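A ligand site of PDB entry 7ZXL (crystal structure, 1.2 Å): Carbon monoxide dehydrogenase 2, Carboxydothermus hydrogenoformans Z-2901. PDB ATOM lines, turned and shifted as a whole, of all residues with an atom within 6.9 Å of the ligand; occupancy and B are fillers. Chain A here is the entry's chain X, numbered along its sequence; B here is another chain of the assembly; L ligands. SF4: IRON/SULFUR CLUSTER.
CA of Gly 68 touches S2 of the ligand, at 3.9 Å. Ile 69 touches the ligand. Ala 72 touches the ligand (CB to S2, 3.98 Å). Met 199 touches the ligand (CG to S1, 3.6 Å). Hydrophobic or aromatic side chains that line the ligand: Ile 69, Ala 72 and Met 199. Along chain A the residues within 4 Å of the ligand span positions 48 to 199. The nearest printed residue that does not touch the ligand is Arg 49 (4.1 Å).
N of Gly 54 sits close to S4 of the ligand, at 3.7 Å. The backbone NH (N) of Cys 70 lies close to a sulfur (S3) of the ligand. The side-chain sulfur (SG) of Cys 56 binds an iron atom (FE1) of the ligand. N of His 50 sits close to S4 of the ligand (3.8 Å). The guanidinium group (NH2) of Arg 80 lies close to a sulfur (S1) of the ligand (3.6 Å). The backbone NH (N) of Cys 51 sits close to a sulfur (S4) of the ligand (3.6 Å). FE2 of the ligand is bound by SG of Cys 51 (2.3 Å). FE3 of the ligand is bound by SG of Cys 48 (2.3 Å). NE2 of Gln 53 sits close to S3 of the ligand, at 3.7 Å. An iron atom (FE4) of the ligand is bound by the side-chain sulfur (SG) of Cys 70 (2.3 Å).
The side-chain amide nitrogen of Gln 38 of chain B is in hydrogen-bond range of the backbone carbonyl oxygen of Gln 53, at 2.8 Å. The backbone NH (N) of Ala 72 lies close to the side-chain sulfur (SG) of Cys 70. ND1 of His 50 is in hydrogen-bond range of O of Thr 197 (2.8 Å). The backbone NH (N) of Cys 48 lies within hydrogen-bond range of the backbone carbonyl oxygen (O) of Cys 56 (2.8 Å). The side-chain sulfur of Cys 51 lies close to the backbone NH of Gln 53 (3.4 Å). The guanidinium group (NH2) of Arg 80 sits close to the side-chain sulfur (SG) of Cys 48 (3.4 Å). The backbone carbonyl oxygen of Cys 56 sits close to the side-chain sulfur of Cys 47 (3.7 Å). The backbone NH (N) of His 50 sits close to the side-chain sulfur (SG) of Cys 48, 3.4 Å away.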
ATOM      1  N   CYS A  47      23.122 -26.743 -20.413  1.00  0.00           N
ATOM      2  CA  CYS A  47      23.469 -26.538 -19.011  1.00  0.00           C
ATOM      3  C   CYS A  47      22.645 -25.369 -18.499  1.00  0.00           C
ATOM      4  O   CYS A  47      22.477 -24.358 -19.209  1.00  0.00           O
ATOM      5  CB  CYS A  47      24.952 -26.266 -18.819  1.00  0.00           C
ATOM      6  SG  CYS A  47      25.369 -25.943 -17.082  1.00  0.00           S
ATOM      7  N   CYS A  48      22.155 -25.495 -17.279  1.00  0.00           N
ATOM      8  CA  CYS A  48      21.393 -24.450 -16.614  1.00  0.00           C
ATOM      9  C   CYS A  48      21.861 -24.305 -15.175  1.00  0.00           C
ATOM     10  O   CYS A  48      21.950 -25.290 -14.445  1.00  0.00           O
ATOM     11  CB  CYS A  48      19.908 -24.791 -16.658  1.00  0.00           C
ATOM     12  SG  CYS A  48      18.863 -23.513 -15.849  1.00  0.00           S
ATOM     13  N   ARG A  49      22.090 -23.052 -14.777  1.00  0.00           N
ATOM     14  CA  ARG A  49      22.427 -22.671 -13.408  1.00  0.00           C
ATOM     15  C   ARG A  49      21.485 -21.588 -12.913  1.00  0.00           C
ATOM     16  O   ARG A  49      21.857 -20.746 -12.096  1.00  0.00           O
ATOM     17  CB  ARG A  49      23.893 -22.214 -13.321  1.00  0.00           C
ATOM     18  CG  ARG A  49      24.874 -23.299 -13.680  1.00  0.00           C
ATOM     19  CD  ARG A  49      26.280 -22.774 -13.833  1.00  0.00           C
ATOM     20  NE  ARG A  49      26.731 -22.092 -12.639  1.00  0.00           N
ATOM     21  CZ  ARG A  49      27.723 -21.200 -12.589  1.00  0.00           C
ATOM     22  NH1 ARG A  49      28.380 -20.846 -13.680  1.00  0.00           N
ATOM     23  NH2 ARG A  49      28.053 -20.663 -11.415  1.00  0.00           N
ATOM     24  N   HIS A  50      20.244 -21.581 -13.398  1.00  0.00           N
ATOM     25  CA  HIS A  50      19.297 -20.536 -13.030  1.00  0.00           C
ATOM     26  C   HIS A  50      18.673 -20.700 -11.655  1.00  0.00           C
ATOM     27  O   HIS A  50      17.921 -19.821 -11.231  1.00  0.00           O
ATOM     28  CB  HIS A  50      18.238 -20.353 -14.105  1.00  0.00           C
ATOM     29  CG  HIS A  50      18.757 -19.824 -15.414  1.00  0.00           C
ATOM     30  ND1 HIS A  50      17.944 -19.267 -16.374  1.00  0.00           N
ATOM     31  CD2 HIS A  50      20.014 -19.814 -15.927  1.00  0.00           C
ATOM     32  CE1 HIS A  50      18.685 -18.902 -17.419  1.00  0.00           C
ATOM     33  NE2 HIS A  50      19.940 -19.209 -17.164  1.00  0.00           N
ATOM     34  N   CYS A  51      18.974 -21.775 -10.919  1.00  0.00           N
ATOM     35  CA  CYS A  51      18.644 -21.801  -9.487  1.00  0.00           C
ATOM     36  C   CYS A  51      19.650 -22.663  -8.743  1.00  0.00           C
ATOM     37  O   CYS A  51      20.501 -23.318  -9.343  1.00  0.00           O
ATOM     38  CB  CYS A  51      17.208 -22.286  -9.262  1.00  0.00           C
ATOM     39  SG  CYS A  51      16.979 -24.107  -9.349  1.00  0.00           S
ATOM     40  N   LEU A  52      19.526 -22.659  -7.416  1.00  0.00           N
ATOM     41  CA  LEU A  52      20.481 -23.343  -6.557  1.00  0.00           C
ATOM     42  C   LEU A  52      20.221 -24.850  -6.462  1.00  0.00           C
ATOM     43  O   LEU A  52      20.932 -25.531  -5.720  1.00  0.00           O
ATOM     44  CB  LEU A  52      20.502 -22.690  -5.165  1.00  0.00           C
ATOM     45  CG  LEU A  52      20.890 -21.215  -5.165  1.00  0.00           C
ATOM     46  CD1 LEU A  52      20.819 -20.703  -3.746  1.00  0.00           C
ATOM     47  CD2 LEU A  52      22.292 -21.012  -5.756  1.00  0.00           C
ATOM     48  N   GLN A  53      19.254 -25.378  -7.207  1.00  0.00           N
ATOM     49  CA  GLN A  53      19.182 -26.830  -7.358  1.00  0.00           C
ATOM     50  C   GLN A  53      20.164 -27.335  -8.405  1.00  0.00           C
ATOM     51  O   GLN A  53      20.477 -28.530  -8.412  1.00  0.00           O
ATOM     52  CB  GLN A  53      17.767 -27.304  -7.705  1.00  0.00           C
ATOM     53  CG  GLN A  53      16.819 -27.042  -6.571  1.00  0.00           C
ATOM     54  CD  GLN A  53      15.362 -27.380  -6.812  1.00  0.00           C
ATOM     55  OE1 GLN A  53      14.668 -27.743  -5.876  1.00  0.00           O
ATOM     56  NE2 GLN A  53      14.881 -27.213  -8.042  1.00  0.00           N
ATOM     57  N   GLY A  54      20.651 -26.435  -9.264  1.00  0.00           N
ATOM     58  CA  GLY A  54      21.599 -26.822 -10.276  1.00  0.00           C
ATOM     59  C   GLY A  54      23.008 -26.931  -9.747  1.00  0.00           C
ATOM     60  O   GLY A  54      23.258 -26.848  -8.533  1.00  0.00           O
ATOM     61  N   PRO A  55      23.977 -27.124 -10.646  1.00  0.00           N
ATOM     62  CA  PRO A  55      23.801 -27.087 -12.094  1.00  0.00           C
ATOM     63  C   PRO A  55      23.023 -28.275 -12.639  1.00  0.00           C
ATOM     64  O   PRO A  55      23.205 -29.415 -12.164  1.00  0.00           O
ATOM     65  CB  PRO A  55      25.246 -27.100 -12.593  1.00  0.00           C
ATOM     66  CG  PRO A  55      25.999 -27.837 -11.497  1.00  0.00           C
ATOM     67  CD  PRO A  55      25.359 -27.418 -10.239  1.00  0.00           C
ATOM     68  N   CYS A  56      22.208 -28.004 -13.636  1.00  0.00           N
ATOM     69  CA  CYS A  56      21.544 -29.051 -14.392  1.00  0.00           C
ATOM     70  C   CYS A  56      22.170 -29.124 -15.768  1.00  0.00           C
ATOM     71  O   CYS A  56      22.465 -28.101 -16.375  1.00  0.00           O
ATOM     72  CB  CYS A  56      20.056 -28.756 -14.509  1.00  0.00           C
ATOM     73  SG  CYS A  56      19.167 -28.939 -12.951  1.00  0.00           S
ATOM     74  N   ARG A  57      22.309 -30.325 -16.266  1.00  0.00           N
ATOM     75  CA  ARG A  57      22.834 -30.488 -17.578  1.00  0.00           C
ATOM     76  C   ARG A  57      22.022 -31.671 -18.230  1.00  0.00           C
ATOM     77  O   ARG A  57      21.286 -32.365 -17.544  1.00  0.00           O
ATOM     78  CB  ARG A  57      24.298 -30.966 -17.564  1.00  0.00           C
ATOM     79  CG  ARG A  57      24.453 -32.372 -17.133  1.00  0.00           C
ATOM     80  CD  ARG A  57      25.846 -32.683 -16.656  1.00  0.00           C
ATOM     81  NE  ARG A  57      25.830 -34.079 -16.251  1.00  0.00           N
ATOM     82  CZ  ARG A  57      25.360 -34.536 -15.077  1.00  0.00           C
ATOM     83  NH1 ARG A  57      25.336 -35.835 -14.852  1.00  0.00           N
ATOM     84  NH2 ARG A  57      24.951 -33.685 -14.154  1.00  0.00           N
ATOM     85  N   VAL A  67      16.451 -34.156 -18.669  1.00  0.00           N
ATOM     86  CA  VAL A  67      15.584 -33.033 -18.330  1.00  0.00           C
ATOM     87  C   VAL A  67      16.158 -32.387 -17.080  1.00  0.00           C
ATOM     88  O   VAL A  67      16.802 -33.047 -16.268  1.00  0.00           O
ATOM     89  CB  VAL A  67      14.142 -33.566 -18.151  1.00  0.00           C
ATOM     90  CG1 VAL A  67      14.081 -34.586 -17.041  1.00  0.00           C
ATOM     91  CG2 VAL A  67      13.169 -32.467 -17.946  1.00  0.00           C
ATOM     92  N   GLY A  68      15.938 -31.083 -16.944  1.00  0.00           N
ATOM     93  CA  GLY A  68      16.360 -30.406 -15.735  1.00  0.00           C
ATOM     94  C   GLY A  68      15.580 -30.849 -14.516  1.00  0.00           C
ATOM     95  O   GLY A  68      14.492 -31.429 -14.609  1.00  0.00           O
ATOM     96  N   ILE A  69      16.124 -30.515 -13.347  1.00  0.00           N
ATOM     97  CA  ILE A  69      15.517 -30.967 -12.092  1.00  0.00           C
ATOM     98  C   ILE A  69      14.087 -30.469 -11.941  1.00  0.00           C
ATOM     99  O   ILE A  69      13.201 -31.211 -11.503  1.00  0.00           O
ATOM    100  CB  ILE A  69      16.425 -30.594 -10.900  1.00  0.00           C
ATOM    101  CG1 ILE A  69      17.652 -31.498 -10.915  1.00  0.00           C
ATOM    102  CG2 ILE A  69      15.640 -30.676  -9.588  1.00  0.00           C
ATOM    103  CD1 ILE A  69      18.726 -31.093  -9.963  1.00  0.00           C
ATOM    104  N   CYS A  70      13.829 -29.210 -12.303  1.00  0.00           N
ATOM    105  CA  CYS A  70      12.497 -28.636 -12.203  1.00  0.00           C
ATOM    106  C   CYS A  70      11.569 -29.077 -13.336  1.00  0.00           C
ATOM    107  O   CYS A  70      10.386 -28.684 -13.335  1.00  0.00           O
ATOM    108  CB  CYS A  70      12.611 -27.118 -12.247  1.00  0.00           C
ATOM    109  SG  CYS A  70      13.329 -26.516 -13.815  1.00  0.00           S
ATOM    110  N   GLY A  71      12.057 -29.873 -14.296  1.00  0.00           N
ATOM    111  CA  GLY A  71      11.287 -30.238 -15.469  1.00  0.00           C
ATOM    112  C   GLY A  71      11.636 -29.461 -16.723  1.00  0.00           C
ATOM    113  O   GLY A  71      11.044 -29.729 -17.779  1.00  0.00           O
ATOM    114  N   ALA A  72      12.589 -28.532 -16.649  1.00  0.00           N
ATOM    115  CA  ALA A  72      12.933 -27.746 -17.843  1.00  0.00           C
ATOM    116  C   ALA A  72      13.530 -28.654 -18.910  1.00  0.00           C
ATOM    117  O   ALA A  72      14.499 -29.356 -18.681  1.00  0.00           O
ATOM    118  CB  ALA A  72      13.925 -26.647 -17.454  1.00  0.00           C
ATOM    119  N   THR A  73      12.962 -28.591 -20.109  1.00  0.00           N
ATOM    120  CA  THR A  73      13.414 -29.396 -21.215  1.00  0.00           C
ATOM    121  C   THR A  73      14.651 -28.759 -21.859  1.00  0.00           C
ATOM    122  O   THR A  73      15.018 -27.614 -21.584  1.00  0.00           O
ATOM    123  CB  THR A  73      12.337 -29.473 -22.275  1.00  0.00           C
ATOM    124  OG1 THR A  73      12.060 -28.145 -22.721  1.00  0.00           O
ATOM    125  CG2 THR A  73      11.049 -30.160 -21.791  1.00  0.00           C
ATOM    126  N   ILE A  77      15.823 -24.843 -21.695  1.00  0.00           N
ATOM    127  CA  ILE A  77      17.141 -24.477 -21.202  1.00  0.00           C
ATOM    128  C   ILE A  77      17.913 -23.708 -22.265  1.00  0.00           C
ATOM    129  O   ILE A  77      18.484 -22.646 -22.004  1.00  0.00           O
ATOM    130  CB  ILE A  77      17.885 -25.733 -20.710  1.00  0.00           C
ATOM    131  CG1 ILE A  77      17.266 -26.179 -19.383  1.00  0.00           C
ATOM    132  CG2 ILE A  77      19.353 -25.469 -20.556  1.00  0.00           C
ATOM    133  CD1 ILE A  77      17.752 -27.542 -18.914  1.00  0.00           C
ATOM    134  N   ARG A  80      16.351 -20.188 -22.836  1.00  0.00           N
ATOM    135  CA  ARG A  80      16.563 -19.261 -21.718  1.00  0.00           C
ATOM    136  C   ARG A  80      17.989 -18.759 -21.710  1.00  0.00           C
ATOM    137  O   ARG A  80      18.230 -17.569 -21.481  1.00  0.00           O
ATOM    138  CB  ARG A  80      16.219 -19.934 -20.383  1.00  0.00           C
ATOM    139  CG  ARG A  80      14.720 -20.259 -20.212  1.00  0.00           C
ATOM    140  CD  ARG A  80      14.361 -20.666 -18.806  1.00  0.00           C
ATOM    141  NE  ARG A  80      15.169 -21.761 -18.306  1.00  0.00           N
ATOM    142  CZ  ARG A  80      14.837 -22.462 -17.223  1.00  0.00           C
ATOM    143  NH1 ARG A  80      13.714 -22.183 -16.582  1.00  0.00           N
ATOM    144  NH2 ARG A  80      15.595 -23.472 -16.805  1.00  0.00           N
ATOM    145  N   THR A 197      13.143 -15.781 -17.778  1.00  0.00           N
ATOM    146  CA  THR A 197      14.106 -16.863 -17.871  1.00  0.00           C
ATOM    147  C   THR A 197      14.522 -17.395 -16.508  1.00  0.00           C
ATOM    148  O   THR A 197      15.264 -18.380 -16.455  1.00  0.00           O
ATOM    149  CB  THR A 197      15.370 -16.428 -18.644  1.00  0.00           C
ATOM    150  OG1 THR A 197      15.979 -15.298 -17.999  1.00  0.00           O
ATOM    151  CG2 THR A 197      15.050 -16.106 -20.095  1.00  0.00           C
ATOM    152  N   SER A 198      14.076 -16.757 -15.420  1.00  0.00           N
ATOM    153  CA  SER A 198      14.342 -17.281 -14.097  1.00  0.00           C
ATOM    154  C   SER A 198      13.516 -18.537 -13.837  1.00  0.00           C
ATOM    155  O   SER A 198      12.635 -18.893 -14.609  1.00  0.00           O
ATOM    156  CB  SER A 198      14.133 -16.195 -13.031  1.00  0.00           C
ATOM    157  OG  SER A 198      12.763 -15.927 -12.798  1.00  0.00           O
ATOM    158  N   MET A 199      13.870 -19.252 -12.774  1.00  0.00           N
ATOM    159  CA  MET A 199      13.285 -20.559 -12.546  1.00  0.00           C
ATOM    160  C   MET A 199      11.759 -20.467 -12.417  1.00  0.00           C
ATOM    161  O   MET A 199      11.222 -19.573 -11.733  1.00  0.00           O
ATOM    162  CB  MET A 199      13.907 -21.219 -11.315  1.00  0.00           C
ATOM    163  CG  MET A 199      13.372 -22.613 -11.016  1.00  0.00           C
ATOM    164  SD  MET A 199      11.824 -22.542 -10.050  1.00  0.00           S
ATOM    165  CE  MET A 199      11.061 -24.073 -10.588  1.00  0.00           C
ATOM    166  N   GLY A 200      11.068 -21.402 -13.057  1.00  0.00           N
ATOM    167  CA  GLY A 200       9.649 -21.547 -12.863  1.00  0.00           C
ATOM    168  C   GLY A 200       8.814 -20.479 -13.518  1.00  0.00           C
ATOM    169  O   GLY A 200       7.671 -20.245 -13.104  1.00  0.00           O
ATOM    170  N   VAL B  28      10.308 -34.462  -9.112  1.00  0.00           N
ATOM    171  CA  VAL B  28      11.495 -33.633  -8.943  1.00  0.00           C
ATOM    172  C   VAL B  28      12.628 -34.415  -8.275  1.00  0.00           C
ATOM    173  O   VAL B  28      13.812 -34.228  -8.610  1.00  0.00           O
ATOM    174  CB  VAL B  28      11.123 -32.353  -8.174  1.00  0.00           C
ATOM    175  CG1 VAL B  28      10.620 -32.656  -6.744  1.00  0.00           C
ATOM    176  CG2 VAL B  28      12.295 -31.397  -8.145  1.00  0.00           C
ATOM    177  N   MET B  35      20.370 -36.535 -12.073  1.00  0.00           N
ATOM    178  CA  MET B  35      21.344 -35.482 -12.318  1.00  0.00           C
ATOM    179  C   MET B  35      22.662 -35.707 -11.572  1.00  0.00           C
ATOM    180  O   MET B  35      23.650 -35.046 -11.887  1.00  0.00           O
ATOM    181  CB  MET B  35      20.759 -34.114 -11.920  1.00  0.00           C
ATOM    182  CG  MET B  35      21.445 -32.924 -12.549  1.00  0.00           C
ATOM    183  SD  MET B  35      21.369 -32.902 -14.355  1.00  0.00           S
ATOM    184  CE  MET B  35      19.633 -32.583 -14.610  1.00  0.00           C
ATOM    185  N   GLN B  38      26.368 -33.948  -9.758  1.00  0.00           N
ATOM    186  CA  GLN B  38      26.258 -32.667 -10.418  1.00  0.00           C
ATOM    187  C   GLN B  38      27.632 -32.057 -10.675  1.00  0.00           C
ATOM    188  O   GLN B  38      28.616 -32.408 -10.041  1.00  0.00           O
ATOM    189  CB  GLN B  38      25.385 -31.716  -9.586  1.00  0.00           C
ATOM    190  CG  GLN B  38      23.958 -32.162  -9.559  1.00  0.00           C
ATOM    191  CD  GLN B  38      23.051 -31.253  -8.780  1.00  0.00           C
ATOM    192  OE1 GLN B  38      22.940 -31.354  -7.557  1.00  0.00           O
ATOM    193  NE2 GLN B  38      22.391 -30.350  -9.468  1.00  0.00           N
ATOM    194  N   PRO B 336       8.044 -26.671 -14.464  1.00  0.00           N
ATOM    195  CA  PRO B 336       7.333 -26.880 -15.730  1.00  0.00           C
ATOM    196  C   PRO B 336       6.926 -28.332 -15.942  1.00  0.00           C
ATOM    197  O   PRO B 336       6.096 -28.604 -16.810  1.00  0.00           O
ATOM    198  CB  PRO B 336       8.284 -26.332 -16.791  1.00  0.00           C
ATOM    199  CG  PRO B 336       9.616 -26.425 -16.140  1.00  0.00           C
ATOM    200  CD  PRO B 336       9.382 -26.115 -14.700  1.00  0.00           C
ATOM    201  N   MET B 560      16.548 -21.669  -2.997  1.00  0.00           N
ATOM    202  CA  MET B 560      16.557 -22.214  -4.352  1.00  0.00           C
ATOM    203  C   MET B 560      16.599 -21.125  -5.424  1.00  0.00           C
ATOM    204  O   MET B 560      17.499 -21.105  -6.260  1.00  0.00           O
ATOM    205  CB  MET B 560      15.344 -23.159  -4.558  1.00  0.00           C
ATOM    206  CG  MET B 560      15.201 -23.777  -5.945  1.00  0.00           C
ATOM    207  SD  MET B 560      14.207 -22.830  -7.104  1.00  0.00           S
ATOM    208  CE  MET B 560      12.606 -22.787  -6.311  1.00  0.00           C
HETATM  209 FE1  SF4 L   1      17.983 -26.964 -12.869  1.00  0.00          FE
HETATM  210 FE2  SF4 L   1      17.186 -24.752 -11.506  1.00  0.00          FE
HETATM  211 FE3  SF4 L   1      17.818 -24.633 -14.147  1.00  0.00          FE
HETATM  212 FE4  SF4 L   1      15.510 -25.909 -13.431  1.00  0.00          FE
HETATM  213  S1  SF4 L   1      16.032 -23.666 -13.211  1.00  0.00           S
HETATM  214  S2  SF4 L   1      17.009 -26.635 -14.933  1.00  0.00           S
HETATM  215  S3  SF4 L   1      16.257 -26.874 -11.463  1.00  0.00           S
HETATM  216  S4  SF4 L   1      19.226 -25.092 -12.411  1.00  0.00           S
